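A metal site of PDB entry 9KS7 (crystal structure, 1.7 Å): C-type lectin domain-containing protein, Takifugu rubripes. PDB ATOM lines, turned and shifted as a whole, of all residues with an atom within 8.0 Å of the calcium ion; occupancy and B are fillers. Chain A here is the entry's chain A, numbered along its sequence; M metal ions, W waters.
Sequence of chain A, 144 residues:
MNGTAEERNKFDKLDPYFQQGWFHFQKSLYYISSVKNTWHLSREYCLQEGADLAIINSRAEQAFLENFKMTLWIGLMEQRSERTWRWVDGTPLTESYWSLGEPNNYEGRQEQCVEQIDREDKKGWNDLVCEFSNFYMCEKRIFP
The calcium ion is bound by O of Ile 55 (2.2 Å). The calcium ion is bound by the side-chain amide oxygen (OD1) of Asn 57 (2.3 Å). The calcium ion is bound by water W1 (2.4 Å). Water W2 is bound to the calcium ion, 2.4 Å away. The calcium ion is bound by OE2 of Glu 139, at 2.5 Å. The side-chain carboxylate (OE2) of Glu 61 is bound to the calcium ion (2.5 Å). The calcium ion is bound by the side-chain carboxylate (OE1) of Glu 139 (2.6 Å). The side-chain carboxylate (OE1) of Glu 61 is bound to the calcium ion.
Four residues have an atom within 4 Å of the calcium ion: Ile 55, Asn 57, Glu 61 and Glu 139.
The side-chain carboxylate (OE2) of Glu 139 lies close to the side-chain hydroxyl (OH) of Tyr 30, at 3.3 Å. The side-chain carboxylate (OE2) of Glu 139 lies close to the side-chain hydroxyl (OG) of Ser 28, 2.6 Å away. The side-chain hydroxyl of Tyr 30 sits close to the side-chain carboxylate of Glu 61, at 2.5 Å. N of Glu 61 lies within hydrogen-bond range of OG of Ser 58, at 3.1 Å.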
ATOM      1  N   PHE A  25      20.317  13.953 -20.382  1.00  0.00           N
ATOM      2  CA  PHE A  25      20.482  15.313 -20.865  1.00  0.00           C
ATOM      3  C   PHE A  25      19.095  15.966 -20.865  1.00  0.00           C
ATOM      4  O   PHE A  25      18.133  15.407 -21.413  1.00  0.00           O
ATOM      5  CB  PHE A  25      21.151  15.297 -22.272  1.00  0.00           C
ATOM      6  CG  PHE A  25      21.232  16.642 -22.916  1.00  0.00           C
ATOM      7  CD1 PHE A  25      22.270  17.521 -22.596  1.00  0.00           C
ATOM      8  CD2 PHE A  25      20.281  17.033 -23.862  1.00  0.00           C
ATOM      9  CE1 PHE A  25      22.347  18.780 -23.212  1.00  0.00           C
ATOM     10  CE2 PHE A  25      20.353  18.294 -24.470  1.00  0.00           C
ATOM     11  CZ  PHE A  25      21.380  19.154 -24.152  1.00  0.00           C
ATOM     12  N   GLN A  26      18.978  17.119 -20.197  1.00  0.00           N
ATOM     13  CA  GLN A  26      17.712  17.865 -20.039  1.00  0.00           C
ATOM     14  C   GLN A  26      16.686  16.950 -19.382  1.00  0.00           C
ATOM     15  O   GLN A  26      16.882  16.560 -18.216  1.00  0.00           O
ATOM     16  CB  GLN A  26      17.285  18.452 -21.389  1.00  0.00           C
ATOM     17  CG  GLN A  26      18.240  19.502 -21.916  1.00  0.00           C
ATOM     18  CD  GLN A  26      17.729  20.173 -23.168  1.00  0.00           C
ATOM     19  OE1 GLN A  26      17.240  19.523 -24.103  1.00  0.00           O
ATOM     20  NE2 GLN A  26      17.814  21.489 -23.182  1.00  0.00           N
ATOM     21  N   LYS A  27      15.584  16.612 -20.035  1.00  0.00           N
ATOM     22  CA  LYS A  27      14.564  15.812 -19.375  1.00  0.00           C
ATOM     23  C   LYS A  27      14.566  14.370 -19.835  1.00  0.00           C
ATOM     24  O   LYS A  27      13.651  13.616 -19.481  1.00  0.00           O
ATOM     25  CB  LYS A  27      13.191  16.436 -19.602  1.00  0.00           C
ATOM     26  CG  LYS A  27      13.142  17.907 -19.228  1.00  0.00           C
ATOM     27  CD  LYS A  27      11.711  18.358 -18.968  1.00  0.00           C
ATOM     28  CE  LYS A  27      11.662  19.805 -18.503  1.00  0.00           C
ATOM     29  NZ  LYS A  27      10.275  20.316 -18.423  1.00  0.00           N
ATOM     30  N   SER A  28      15.584  13.952 -20.582  1.00  0.00           N
ATOM     31  CA  SER A  28      15.550  12.677 -21.274  1.00  0.00           C
ATOM     32  C   SER A  28      16.764  11.829 -20.931  1.00  0.00           C
ATOM     33  O   SER A  28      17.806  12.332 -20.513  1.00  0.00           O
ATOM     34  CB  SER A  28      15.510  12.876 -22.794  1.00  0.00           C
ATOM     35  OG  SER A  28      14.307  13.520 -23.206  1.00  0.00           O
ATOM     36  N   TYR A  30      19.246   9.036 -22.979  1.00  0.00           N
ATOM     37  CA  TYR A  30      19.621   8.762 -24.352  1.00  0.00           C
ATOM     38  C   TYR A  30      20.482   7.512 -24.397  1.00  0.00           C
ATOM     39  O   TYR A  30      21.191   7.199 -23.434  1.00  0.00           O
ATOM     40  CB  TYR A  30      20.419   9.905 -25.003  1.00  0.00           C
ATOM     41  CG  TYR A  30      19.651  11.197 -25.100  1.00  0.00           C
ATOM     42  CD1 TYR A  30      19.528  12.036 -24.002  1.00  0.00           C
ATOM     43  CD2 TYR A  30      19.026  11.565 -26.288  1.00  0.00           C
ATOM     44  CE1 TYR A  30      18.829  13.252 -24.097  1.00  0.00           C
ATOM     45  CE2 TYR A  30      18.297  12.759 -26.398  1.00  0.00           C
ATOM     46  CZ  TYR A  30      18.217  13.602 -25.285  1.00  0.00           C
ATOM     47  OH  TYR A  30      17.524  14.794 -25.383  1.00  0.00           O
ATOM     48  N   LEU A  53      13.264   6.457 -31.269  1.00  0.00           N
ATOM     49  CA  LEU A  53      14.400   7.174 -31.822  1.00  0.00           C
ATOM     50  C   LEU A  53      14.368   8.638 -31.362  1.00  0.00           C
ATOM     51  O   LEU A  53      13.305   9.173 -31.000  1.00  0.00           O
ATOM     52  CB  LEU A  53      14.376   7.091 -33.355  1.00  0.00           C
ATOM     53  CG  LEU A  53      14.792   5.732 -33.938  1.00  0.00           C
ATOM     54  CD1 LEU A  53      14.551   5.752 -35.430  1.00  0.00           C
ATOM     55  CD2 LEU A  53      16.298   5.456 -33.688  1.00  0.00           C
ATOM     56  N   ALA A  54      15.555   9.254 -31.299  1.00  0.00           N
ATOM     57  CA  ALA A  54      15.681  10.588 -30.718  1.00  0.00           C
ATOM     58  C   ALA A  54      14.822  11.601 -31.483  1.00  0.00           C
ATOM     59  O   ALA A  54      14.759  11.586 -32.716  1.00  0.00           O
ATOM     60  CB  ALA A  54      17.149  11.026 -30.710  1.00  0.00           C
ATOM     61  N   ILE A  55      14.178  12.492 -30.740  1.00  0.00           N
ATOM     62  CA  ILE A  55      13.404  13.595 -31.299  1.00  0.00           C
ATOM     63  C   ILE A  55      14.094  14.903 -30.925  1.00  0.00           C
ATOM     64  O   ILE A  55      14.349  15.173 -29.732  1.00  0.00           O
ATOM     65  CB  ILE A  55      11.966  13.576 -30.783  1.00  0.00           C
ATOM     66  CG1 ILE A  55      11.238  12.336 -31.294  1.00  0.00           C
ATOM     67  CG2 ILE A  55      11.220  14.853 -31.227  1.00  0.00           C
ATOM     68  CD1 ILE A  55       9.953  12.044 -30.482  1.00  0.00           C
ATOM     69  N   ILE A  56      14.437  15.709 -31.936  1.00  0.00           N
ATOM     70  CA  ILE A  56      15.189  16.936 -31.698  1.00  0.00           C
ATOM     71  C   ILE A  56      14.202  18.088 -31.494  1.00  0.00           C
ATOM     72  O   ILE A  56      13.489  18.476 -32.428  1.00  0.00           O
ATOM     73  CB  ILE A  56      16.151  17.237 -32.846  1.00  0.00           C
ATOM     74  CG1 ILE A  56      17.049  16.019 -33.094  1.00  0.00           C
ATOM     75  CG2 ILE A  56      16.973  18.525 -32.515  1.00  0.00           C
ATOM     76  CD1 ILE A  56      17.777  15.540 -31.838  1.00  0.00           C
ATOM     77  N   ASN A  57      14.183  18.635 -30.275  1.00  0.00           N
ATOM     78  CA  ASN A  57      13.193  19.629 -29.856  1.00  0.00           C
ATOM     79  C   ASN A  57      13.772  21.019 -29.622  1.00  0.00           C
ATOM     80  O   ASN A  57      12.993  21.937 -29.351  1.00  0.00           O
ATOM     81  CB  ASN A  57      12.512  19.190 -28.552  1.00  0.00           C
ATOM     82  CG  ASN A  57      11.806  17.881 -28.706  1.00  0.00           C
ATOM     83  OD1 ASN A  57      12.328  16.827 -28.336  1.00  0.00           O
ATOM     84  ND2 ASN A  57      10.603  17.933 -29.255  1.00  0.00           N
ATOM     85  N   SER A  58      15.092  21.191 -29.702  1.00  0.00           N
ATOM     86  CA  SER A  58      15.693  22.477 -29.382  1.00  0.00           C
ATOM     87  C   SER A  58      17.062  22.580 -30.023  1.00  0.00           C
ATOM     88  O   SER A  58      17.681  21.582 -30.393  1.00  0.00           O
ATOM     89  CB  SER A  58      15.795  22.700 -27.865  1.00  0.00           C
ATOM     90  OG  SER A  58      16.779  21.851 -27.272  1.00  0.00           O
ATOM     91  N   GLU A  61      19.538  20.674 -28.005  1.00  0.00           N
ATOM     92  CA  GLU A  61      19.510  19.224 -28.204  1.00  0.00           C
ATOM     93  C   GLU A  61      20.164  18.850 -29.529  1.00  0.00           C
ATOM     94  O   GLU A  61      20.855  17.818 -29.613  1.00  0.00           O
ATOM     95  CB  GLU A  61      18.076  18.707 -28.135  1.00  0.00           C
ATOM     96  CG  GLU A  61      18.003  17.165 -28.051  1.00  0.00           C
ATOM     97  CD  GLU A  61      16.591  16.685 -27.866  1.00  0.00           C
ATOM     98  OE1 GLU A  61      15.647  17.489 -28.118  1.00  0.00           O
ATOM     99  OE2 GLU A  61      16.418  15.499 -27.463  1.00  0.00           O
ATOM    100  N   TRP A  87       7.907  13.485 -36.756  1.00  0.00           N
ATOM    101  CA  TRP A  87       8.688  12.783 -35.732  1.00  0.00           C
ATOM    102  C   TRP A  87       7.975  11.497 -35.310  1.00  0.00           C
ATOM    103  O   TRP A  87       6.785  11.312 -35.556  1.00  0.00           O
ATOM    104  CB  TRP A  87       8.944  13.676 -34.505  1.00  0.00           C
ATOM    105  CG  TRP A  87       9.766  14.896 -34.804  1.00  0.00           C
ATOM    106  CD1 TRP A  87       9.328  16.177 -35.010  1.00  0.00           C
ATOM    107  CD2 TRP A  87      11.191  14.921 -34.953  1.00  0.00           C
ATOM    108  NE1 TRP A  87      10.408  17.010 -35.272  1.00  0.00           N
ATOM    109  CE2 TRP A  87      11.559  16.252 -35.235  1.00  0.00           C
ATOM    110  CE3 TRP A  87      12.198  13.948 -34.842  1.00  0.00           C
ATOM    111  CZ2 TRP A  87      12.886  16.636 -35.430  1.00  0.00           C
ATOM    112  CZ3 TRP A  87      13.517  14.326 -35.041  1.00  0.00           C
ATOM    113  CH2 TRP A  87      13.850  15.659 -35.334  1.00  0.00           C
ATOM    114  N   ASP A  89       6.947  10.454 -32.616  1.00  0.00           N
ATOM    115  CA  ASP A  89       5.857  10.631 -31.657  1.00  0.00           C
ATOM    116  C   ASP A  89       4.614  11.222 -32.315  1.00  0.00           C
ATOM    117  O   ASP A  89       3.630  11.519 -31.617  1.00  0.00           O
ATOM    118  CB  ASP A  89       6.296  11.497 -30.461  1.00  0.00           C
ATOM    119  CG  ASP A  89       6.594  12.951 -30.841  1.00  0.00           C
ATOM    120  OD1 ASP A  89       6.662  13.278 -32.037  1.00  0.00           O
ATOM    121  OD2 ASP A  89       6.798  13.770 -29.912  1.00  0.00           O
ATOM    122  N   GLU A 139      15.876   7.944 -27.509  1.00  0.00           N
ATOM    123  CA  GLU A 139      15.608   8.940 -26.492  1.00  0.00           C
ATOM    124  C   GLU A 139      14.383   8.493 -25.704  1.00  0.00           C
ATOM    125  O   GLU A 139      13.381   8.103 -26.291  1.00  0.00           O
ATOM    126  CB  GLU A 139      15.332  10.329 -27.078  1.00  0.00           C
ATOM    127  CG  GLU A 139      15.029  11.374 -26.009  1.00  0.00           C
ATOM    128  CD  GLU A 139      14.634  12.721 -26.591  1.00  0.00           C
ATOM    129  OE1 GLU A 139      14.501  12.849 -27.840  1.00  0.00           O
ATOM    130  OE2 GLU A 139      14.463  13.661 -25.790  1.00  0.00           O
ATOM    131  N   LYS A 140      14.469   8.615 -24.382  1.00  0.00           N
ATOM    132  CA  LYS A 140      13.354   8.312 -23.492  1.00  0.00           C
ATOM    133  C   LYS A 140      13.127   9.561 -22.638  1.00  0.00           C
ATOM    134  O   LYS A 140      13.933   9.855 -21.756  1.00  0.00           O
ATOM    135  CB  LYS A 140      13.670   7.109 -22.617  1.00  0.00           C
ATOM    136  CG  LYS A 140      12.559   6.659 -21.728  1.00  0.00           C
ATOM    137  CD  LYS A 140      13.120   5.730 -20.678  1.00  0.00           C
ATOM    138  CE  LYS A 140      12.021   4.990 -19.973  1.00  0.00           C
ATOM    139  NZ  LYS A 140      11.702   3.672 -20.649  1.00  0.00           N
ATOM    140  N   ARG A 141      12.054  10.287 -22.921  1.00  0.00           N
ATOM    141  CA  ARG A 141      11.701  11.469 -22.148  1.00  0.00           C
ATOM    142  C   ARG A 141      11.151  10.982 -20.820  1.00  0.00           C
ATOM    143  O   ARG A 141      10.066  10.411 -20.776  1.00  0.00           O
ATOM    144  CB  ARG A 141      10.682  12.304 -22.919  1.00  0.00           C
ATOM    145  CG  ARG A 141      10.560  13.768 -22.493  1.00  0.00           C
ATOM    146  CD  ARG A 141       9.731  13.906 -21.219  1.00  0.00           C
ATOM    147  NE  ARG A 141       9.362  15.270 -20.874  1.00  0.00           N
ATOM    148  CZ  ARG A 141       8.625  16.090 -21.626  1.00  0.00           C
ATOM    149  NH1 ARG A 141       8.111  15.692 -22.780  1.00  0.00           N
ATOM    150  NH2 ARG A 141       8.398  17.333 -21.197  1.00  0.00           N
HETATM  151 CA    CA M   1      13.936  15.321 -27.551  1.00  0.00          CA
HETATM  152  O   HOH W   1      11.836  14.277 -27.160  1.00  0.00           O
HETATM  153  O   HOH W   2      13.786  16.807 -25.614  1.00  0.00           O
